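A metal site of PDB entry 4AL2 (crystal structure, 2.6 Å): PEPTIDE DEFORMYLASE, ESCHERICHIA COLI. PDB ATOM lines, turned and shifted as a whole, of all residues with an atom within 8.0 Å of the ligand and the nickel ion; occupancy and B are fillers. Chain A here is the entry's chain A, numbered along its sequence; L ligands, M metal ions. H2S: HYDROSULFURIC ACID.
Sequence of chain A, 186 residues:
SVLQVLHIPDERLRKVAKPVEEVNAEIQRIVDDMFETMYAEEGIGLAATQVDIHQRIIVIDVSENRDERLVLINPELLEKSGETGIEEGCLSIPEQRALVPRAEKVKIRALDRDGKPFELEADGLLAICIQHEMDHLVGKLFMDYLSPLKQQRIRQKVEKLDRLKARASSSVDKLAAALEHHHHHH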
ATOM      1  N   VAL A   5       1.628  11.860  -1.466  1.00  0.00           N
ATOM      2  CA  VAL A   5       0.317  11.328  -1.846  1.00  0.00           C
ATOM      3  C   VAL A   5       0.350   9.798  -1.815  1.00  0.00           C
ATOM      4  O   VAL A   5       1.155   9.187  -2.487  1.00  0.00           O
ATOM      5  CB  VAL A   5      -0.150  11.828  -3.234  1.00  0.00           C
ATOM      6  CG1 VAL A   5      -1.385  11.067  -3.687  1.00  0.00           C
ATOM      7  CG2 VAL A   5      -0.436  13.324  -3.210  1.00  0.00           C
ATOM      8  N   LEU A  13      -6.218   4.472   1.781  1.00  0.00           N
ATOM      9  CA  LEU A  13      -7.072   5.042   0.720  1.00  0.00           C
ATOM     10  C   LEU A  13      -8.494   4.508   0.816  1.00  0.00           C
ATOM     11  O   LEU A  13      -9.413   5.048   0.176  1.00  0.00           O
ATOM     12  CB  LEU A  13      -6.512   4.776  -0.672  1.00  0.00           C
ATOM     13  CG  LEU A  13      -5.246   5.545  -0.969  1.00  0.00           C
ATOM     14  CD1 LEU A  13      -4.465   4.868  -2.085  1.00  0.00           C
ATOM     15  CD2 LEU A  13      -5.596   6.979  -1.301  1.00  0.00           C
ATOM     16  N   MET A  38      -1.512  19.486  -4.790  1.00  0.00           N
ATOM     17  CA  MET A  38      -2.256  19.242  -6.009  1.00  0.00           C
ATOM     18  C   MET A  38      -1.598  19.839  -7.253  1.00  0.00           C
ATOM     19  O   MET A  38      -1.349  19.115  -8.214  1.00  0.00           O
ATOM     20  CB  MET A  38      -3.682  19.696  -5.871  1.00  0.00           C
ATOM     21  CG  MET A  38      -4.492  19.347  -7.080  1.00  0.00           C
ATOM     22  SD  MET A  38      -5.907  20.436  -7.067  1.00  0.00           S
ATOM     23  CE  MET A  38      -5.158  21.918  -7.720  1.00  0.00           C
ATOM     24  N   GLY A  43      -2.286  17.940 -10.779  1.00  0.00           N
ATOM     25  CA  GLY A  43      -3.583  17.286 -10.657  1.00  0.00           C
ATOM     26  C   GLY A  43      -4.693  18.320 -10.603  1.00  0.00           C
ATOM     27  O   GLY A  43      -4.434  19.495 -10.309  1.00  0.00           O
ATOM     28  N   ILE A  44      -5.921  17.904 -10.890  1.00  0.00           N
ATOM     29  CA  ILE A  44      -7.020  18.861 -10.992  1.00  0.00           C
ATOM     30  C   ILE A  44      -7.922  18.804  -9.765  1.00  0.00           C
ATOM     31  O   ILE A  44      -8.847  19.600  -9.648  1.00  0.00           O
ATOM     32  CB  ILE A  44      -7.860  18.645 -12.266  1.00  0.00           C
ATOM     33  CG1 ILE A  44      -8.646  17.312 -12.160  1.00  0.00           C
ATOM     34  CG2 ILE A  44      -6.955  18.788 -13.491  1.00  0.00           C
ATOM     35  CD1 ILE A  44      -9.128  16.693 -13.455  1.00  0.00           C
ATOM     36  N   GLY A  45      -7.631  17.865  -8.864  1.00  0.00           N
ATOM     37  CA  GLY A  45      -8.386  17.712  -7.614  1.00  0.00           C
ATOM     38  C   GLY A  45      -7.632  16.840  -6.630  1.00  0.00           C
ATOM     39  O   GLY A  45      -6.772  16.052  -7.042  1.00  0.00           O
ATOM     40  N   LEU A  46      -7.941  17.013  -5.325  1.00  0.00           N
ATOM     41  CA  LEU A  46      -7.301  16.258  -4.237  1.00  0.00           C
ATOM     42  C   LEU A  46      -8.208  16.124  -3.023  1.00  0.00           C
ATOM     43  O   LEU A  46      -8.940  17.058  -2.680  1.00  0.00           O
ATOM     44  CB  LEU A  46      -5.968  16.880  -3.822  1.00  0.00           C
ATOM     45  CG  LEU A  46      -4.993  16.053  -2.968  1.00  0.00           C
ATOM     46  CD1 LEU A  46      -4.285  14.924  -3.709  1.00  0.00           C
ATOM     47  CD2 LEU A  46      -3.966  16.995  -2.369  1.00  0.00           C
ATOM     48  N   ALA A  47      -8.164  14.957  -2.379  1.00  0.00           N
ATOM     49  CA  ALA A  47      -8.931  14.712  -1.170  1.00  0.00           C
ATOM     50  C   ALA A  47      -8.014  14.347   0.008  1.00  0.00           C
ATOM     51  O   ALA A  47      -7.084  13.550  -0.146  1.00  0.00           O
ATOM     52  CB  ALA A  47      -9.945  13.619  -1.422  1.00  0.00           C
ATOM     53  N   GLN A  50      -6.153  11.102   0.584  1.00  0.00           N
ATOM     54  CA  GLN A  50      -5.035  10.734  -0.261  1.00  0.00           C
ATOM     55  C   GLN A  50      -3.730  11.196   0.297  1.00  0.00           C
ATOM     56  O   GLN A  50      -2.698  10.624  -0.032  1.00  0.00           O
ATOM     57  CB  GLN A  50      -5.184  11.387  -1.626  1.00  0.00           C
ATOM     58  CG  GLN A  50      -6.494  11.054  -2.318  1.00  0.00           C
ATOM     59  CD  GLN A  50      -6.531  11.609  -3.708  1.00  0.00           C
ATOM     60  OE1 GLN A  50      -7.263  12.563  -3.988  1.00  0.00           O
ATOM     61  NE2 GLN A  50      -5.726  11.025  -4.608  1.00  0.00           N
ATOM     62  N   VAL A  59      -9.919  19.897  -2.316  1.00  0.00           N
ATOM     63  CA  VAL A  59      -9.484  21.079  -3.096  1.00  0.00           C
ATOM     64  C   VAL A  59      -9.511  20.749  -4.585  1.00  0.00           C
ATOM     65  O   VAL A  59      -9.135  19.657  -4.978  1.00  0.00           O
ATOM     66  CB  VAL A  59      -8.096  21.621  -2.667  1.00  0.00           C
ATOM     67  CG1 VAL A  59      -8.092  22.068  -1.211  1.00  0.00           C
ATOM     68  CG2 VAL A  59      -6.987  20.615  -2.903  1.00  0.00           C
ATOM     69  N   GLU A  88     -10.501   9.382 -16.938  1.00  0.00           N
ATOM     70  CA  GLU A  88     -10.079   9.939 -15.662  1.00  0.00           C
ATOM     71  C   GLU A  88      -8.712   9.409 -15.220  1.00  0.00           C
ATOM     72  O   GLU A  88      -8.339   8.275 -15.528  1.00  0.00           O
ATOM     73  CB  GLU A  88     -11.105   9.616 -14.572  1.00  0.00           C
ATOM     74  CG  GLU A  88     -12.450  10.306 -14.714  1.00  0.00           C
ATOM     75  CD  GLU A  88     -13.323  10.130 -13.490  1.00  0.00           C
ATOM     76  OE1 GLU A  88     -12.809   9.876 -12.387  1.00  0.00           O
ATOM     77  OE2 GLU A  88     -14.558  10.251 -13.644  1.00  0.00           O
ATOM     78  N   GLY A  89      -7.987  10.247 -14.478  1.00  0.00           N
ATOM     79  CA  GLY A  89      -6.747   9.838 -13.813  1.00  0.00           C
ATOM     80  C   GLY A  89      -6.745  10.102 -12.315  1.00  0.00           C
ATOM     81  O   GLY A  89      -7.633  10.788 -11.788  1.00  0.00           O
ATOM     82  N   CYS A  90      -5.726   9.575 -11.626  1.00  0.00           N
ATOM     83  CA  CYS A  90      -5.660   9.678 -10.168  1.00  0.00           C
ATOM     84  C   CYS A  90      -4.213   9.770  -9.692  1.00  0.00           C
ATOM     85  O   CYS A  90      -3.380   8.944 -10.075  1.00  0.00           O
ATOM     86  CB  CYS A  90      -6.339   8.459  -9.542  1.00  0.00           C
ATOM     87  SG  CYS A  90      -6.662   8.533  -7.768  1.00  0.00           S
ATOM     88  N   LEU A  91      -3.911  10.743  -8.836  1.00  0.00           N
ATOM     89  CA  LEU A  91      -2.565  10.873  -8.255  1.00  0.00           C
ATOM     90  C   LEU A  91      -2.181   9.628  -7.450  1.00  0.00           C
ATOM     91  O   LEU A  91      -1.012   9.229  -7.449  1.00  0.00           O
ATOM     92  CB  LEU A  91      -2.466  12.139  -7.401  1.00  0.00           C
ATOM     93  CG  LEU A  91      -2.624  13.444  -8.191  1.00  0.00           C
ATOM     94  CD1 LEU A  91      -2.554  14.686  -7.298  1.00  0.00           C
ATOM     95  CD2 LEU A  91      -1.587  13.529  -9.310  1.00  0.00           C
ATOM     96  N   SER A  92      -3.186   8.991  -6.826  1.00  0.00           N
ATOM     97  CA  SER A  92      -2.998   7.766  -6.024  1.00  0.00           C
ATOM     98  C   SER A  92      -2.917   6.442  -6.795  1.00  0.00           C
ATOM     99  O   SER A  92      -2.548   5.420  -6.232  1.00  0.00           O
ATOM    100  CB  SER A  92      -4.105   7.675  -4.971  1.00  0.00           C
ATOM    101  OG  SER A  92      -4.086   8.832  -4.133  1.00  0.00           O
ATOM    102  N   ILE A  93      -3.313   6.450  -8.071  1.00  0.00           N
ATOM    103  CA  ILE A  93      -3.156   5.304  -8.978  1.00  0.00           C
ATOM    104  C   ILE A  93      -2.222   5.713 -10.143  1.00  0.00           C
ATOM    105  O   ILE A  93      -2.673   5.942 -11.265  1.00  0.00           O
ATOM    106  CB  ILE A  93      -4.535   4.816  -9.518  1.00  0.00           C
ATOM    107  CG1 ILE A  93      -5.517   4.567  -8.379  1.00  0.00           C
ATOM    108  CG2 ILE A  93      -4.383   3.560 -10.356  1.00  0.00           C
ATOM    109  CD1 ILE A  93      -6.966   4.896  -8.703  1.00  0.00           C
ATOM    110  N   ARG A 102     -20.329   8.745 -14.714  1.00  0.00           N
ATOM    111  CA  ARG A 102     -20.609   9.803 -13.758  1.00  0.00           C
ATOM    112  C   ARG A 102     -21.928  10.397 -14.107  1.00  0.00           C
ATOM    113  O   ARG A 102     -22.364  10.352 -15.267  1.00  0.00           O
ATOM    114  CB  ARG A 102     -19.581  10.937 -13.867  1.00  0.00           C
ATOM    115  CG  ARG A 102     -18.140  10.548 -13.578  1.00  0.00           C
ATOM    116  CD  ARG A 102     -17.926  10.317 -12.097  1.00  0.00           C
ATOM    117  NE  ARG A 102     -16.532   9.966 -11.843  1.00  0.00           N
ATOM    118  CZ  ARG A 102     -16.109   9.359 -10.749  1.00  0.00           C
ATOM    119  NH1 ARG A 102     -16.973   9.020  -9.808  1.00  0.00           N
ATOM    120  NH2 ARG A 102     -14.821   9.086 -10.618  1.00  0.00           N
ATOM    121  N   CYS A 129     -15.215  15.964 -11.682  1.00  0.00           N
ATOM    122  CA  CYS A 129     -14.205  16.148 -10.651  1.00  0.00           C
ATOM    123  C   CYS A 129     -14.737  16.181  -9.206  1.00  0.00           C
ATOM    124  O   CYS A 129     -14.156  15.570  -8.305  1.00  0.00           O
ATOM    125  CB  CYS A 129     -13.375  17.389 -10.928  1.00  0.00           C
ATOM    126  SG  CYS A 129     -11.996  17.536  -9.790  1.00  0.00           S
ATOM    127  N   HIS A 132     -15.441  12.654  -8.365  1.00  0.00           N
ATOM    128  CA  HIS A 132     -14.297  11.765  -8.281  1.00  0.00           C
ATOM    129  C   HIS A 132     -13.663  11.911  -6.950  1.00  0.00           C
ATOM    130  O   HIS A 132     -13.230  10.934  -6.344  1.00  0.00           O
ATOM    131  CB  HIS A 132     -13.357  12.090  -9.429  1.00  0.00           C
ATOM    132  CG  HIS A 132     -11.972  11.531  -9.275  1.00  0.00           C
ATOM    133  ND1 HIS A 132     -11.438  10.736 -10.196  1.00  0.00           N
ATOM    134  CD2 HIS A 132     -11.003  11.752  -8.317  1.00  0.00           C
ATOM    135  CE1 HIS A 132     -10.186  10.429  -9.829  1.00  0.00           C
ATOM    136  NE2 HIS A 132      -9.923  11.058  -8.681  1.00  0.00           N
ATOM    137  N   GLU A 133     -13.643  13.157  -6.472  1.00  0.00           N
ATOM    138  CA  GLU A 133     -12.996  13.518  -5.215  1.00  0.00           C
ATOM    139  C   GLU A 133     -13.822  13.086  -4.002  1.00  0.00           C
ATOM    140  O   GLU A 133     -13.267  12.551  -3.050  1.00  0.00           O
ATOM    141  CB  GLU A 133     -12.689  15.021  -5.180  1.00  0.00           C
ATOM    142  CG  GLU A 133     -11.674  15.435  -6.229  1.00  0.00           C
ATOM    143  CD  GLU A 133     -10.354  14.716  -6.060  1.00  0.00           C
ATOM    144  OE1 GLU A 133     -10.138  14.214  -4.948  1.00  0.00           O
ATOM    145  OE2 GLU A 133      -9.540  14.649  -7.003  1.00  0.00           O
ATOM    146  N   ASP A 135     -15.800  10.568  -3.935  1.00  0.00           N
ATOM    147  CA  ASP A 135     -15.536   9.123  -3.874  1.00  0.00           C
ATOM    148  C   ASP A 135     -14.309   8.780  -2.971  1.00  0.00           C
ATOM    149  O   ASP A 135     -14.400   7.848  -2.179  1.00  0.00           O
ATOM    150  CB  ASP A 135     -15.350   8.509  -5.276  1.00  0.00           C
ATOM    151  CG  ASP A 135     -16.691   8.115  -5.948  1.00  0.00           C
ATOM    152  OD1 ASP A 135     -17.784   8.357  -5.385  1.00  0.00           O
ATOM    153  OD2 ASP A 135     -16.638   7.552  -7.072  1.00  0.00           O
ATOM    154  N   HIS A 136     -13.207   9.530  -3.092  1.00  0.00           N
ATOM    155  CA  HIS A 136     -12.048   9.360  -2.194  1.00  0.00           C
ATOM    156  C   HIS A 136     -12.414   9.447  -0.749  1.00  0.00           C
ATOM    157  O   HIS A 136     -11.984   8.583  -0.006  1.00  0.00           O
ATOM    158  CB  HIS A 136     -10.955  10.383  -2.439  1.00  0.00           C
ATOM    159  CG  HIS A 136     -10.060  10.076  -3.615  1.00  0.00           C
ATOM    160  ND1 HIS A 136      -9.341   8.939  -3.717  1.00  0.00           N
ATOM    161  CD2 HIS A 136      -9.731  10.854  -4.741  1.00  0.00           C
ATOM    162  CE1 HIS A 136      -8.619   8.957  -4.859  1.00  0.00           C
ATOM    163  NE2 HIS A 136      -8.855  10.126  -5.483  1.00  0.00           N
ATOM    164  N   LYS A 140     -13.699   5.037  -1.793  1.00  0.00           N
ATOM    165  CA  LYS A 140     -13.827   4.592  -3.185  1.00  0.00           C
ATOM    166  C   LYS A 140     -12.866   5.263  -4.186  1.00  0.00           C
ATOM    167  O   LYS A 140     -12.695   6.489  -4.178  1.00  0.00           O
ATOM    168  CB  LYS A 140     -15.277   4.730  -3.659  1.00  0.00           C
ATOM    169  CG  LYS A 140     -15.618   3.899  -4.882  1.00  0.00           C
ATOM    170  CD  LYS A 140     -16.999   4.230  -5.445  1.00  0.00           C
ATOM    171  CE  LYS A 140     -18.060   3.193  -5.091  1.00  0.00           C
ATOM    172  NZ  LYS A 140     -19.022   2.996  -6.236  1.00  0.00           N
ATOM    173  N   LEU A 141     -12.252   4.448  -5.044  1.00  0.00           N
ATOM    174  CA  LEU A 141     -11.358   4.907  -6.114  1.00  0.00           C
ATOM    175  C   LEU A 141     -11.997   4.601  -7.482  1.00  0.00           C
ATOM    176  O   LEU A 141     -12.841   3.699  -7.581  1.00  0.00           O
ATOM    177  CB  LEU A 141     -10.039   4.158  -6.021  1.00  0.00           C
ATOM    178  CG  LEU A 141      -9.288   4.317  -4.706  1.00  0.00           C
ATOM    179  CD1 LEU A 141      -8.506   3.064  -4.389  1.00  0.00           C
ATOM    180  CD2 LEU A 141      -8.344   5.495  -4.833  1.00  0.00           C
ATOM    181  N   PHE A 142     -11.612   5.330  -8.519  1.00  0.00           N
ATOM    182  CA  PHE A 142     -12.275   5.213  -9.815  1.00  0.00           C
ATOM    183  C   PHE A 142     -12.138   3.866 -10.522  1.00  0.00           C
ATOM    184  O   PHE A 142     -12.984   3.502 -11.338  1.00  0.00           O
ATOM    185  CB  PHE A 142     -11.865   6.349 -10.757  1.00  0.00           C
ATOM    186  CG  PHE A 142     -10.589   6.111 -11.493  1.00  0.00           C
ATOM    187  CD1 PHE A 142     -10.591   5.435 -12.702  1.00  0.00           C
ATOM    188  CD2 PHE A 142      -9.381   6.601 -10.989  1.00  0.00           C
ATOM    189  CE1 PHE A 142      -9.414   5.220 -13.390  1.00  0.00           C
ATOM    190  CE2 PHE A 142      -8.196   6.390 -11.692  1.00  0.00           C
ATOM    191  CZ  PHE A 142      -8.226   5.703 -12.897  1.00  0.00           C
HETATM  192  S   H2S L   1      -6.816  12.612  -7.362  1.00  0.00           S
HETATM  193 NI    NI M   1      -8.073  10.355  -7.353  1.00  0.00          NI
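Gln 50 touches the nickel ion. Four residues have an atom within 4 Å of the nickel ion: Gln 50, Cys 90, His 132 and His 136.
NE2 of His 136 binds the nickel ion (2.0 Å). The side-chain sulfur (SG) of Cys 90 binds the nickel ion (2.3 Å). A ring nitrogen (NE2) of His 132 binds the nickel ion (2.4 Å). S of the ligand is bound to the nickel ion (2.6 Å). The nickel ion has four donor atoms within binding distance.
The side-chain carboxylate of Glu 133 lies close to a sulfur (S) of the ligand. O of Gly 45 sits close to S of the ligand (3.5 Å). S of the ligand sits close to NE2 of Gln 50, 3.4 Å away. N of Leu 91 sits close to S of the ligand (3.8 Å).
SG of Cys 90 sits close to N of Ser 92 (3.6 Å). The side-chain carboxylate (OE2) of Glu 133 is in hydrogen-bond range of the backbone NH (N) of Leu 46 (3.3 Å). OE1 of Glu 133 sits at hydrogen-bond distance from N of Ala 47. A ring nitrogen (ND1) of His 132 sits at hydrogen-bond distance from the side-chain carboxylate (OE1) of Glu 88 (2.7 Å). The side-chain hydroxyl (OG) of Ser 92 lies within hydrogen-bond range of the side-chain amide nitrogen (NE2) of Gln 50 (2.8 Å). The side-chain amide oxygen (OE1) of Gln 50 is in hydrogen-bond range of the backbone NH (N) of Ala 47, 3.0 Å away. The side-chain sulfur (SD) of Met 38 is in hydrogen-bond range of the backbone NH (N) of Gly 45, at 3.6 Å. NE2 of His 136 sits close to OE1 of Gln 50.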
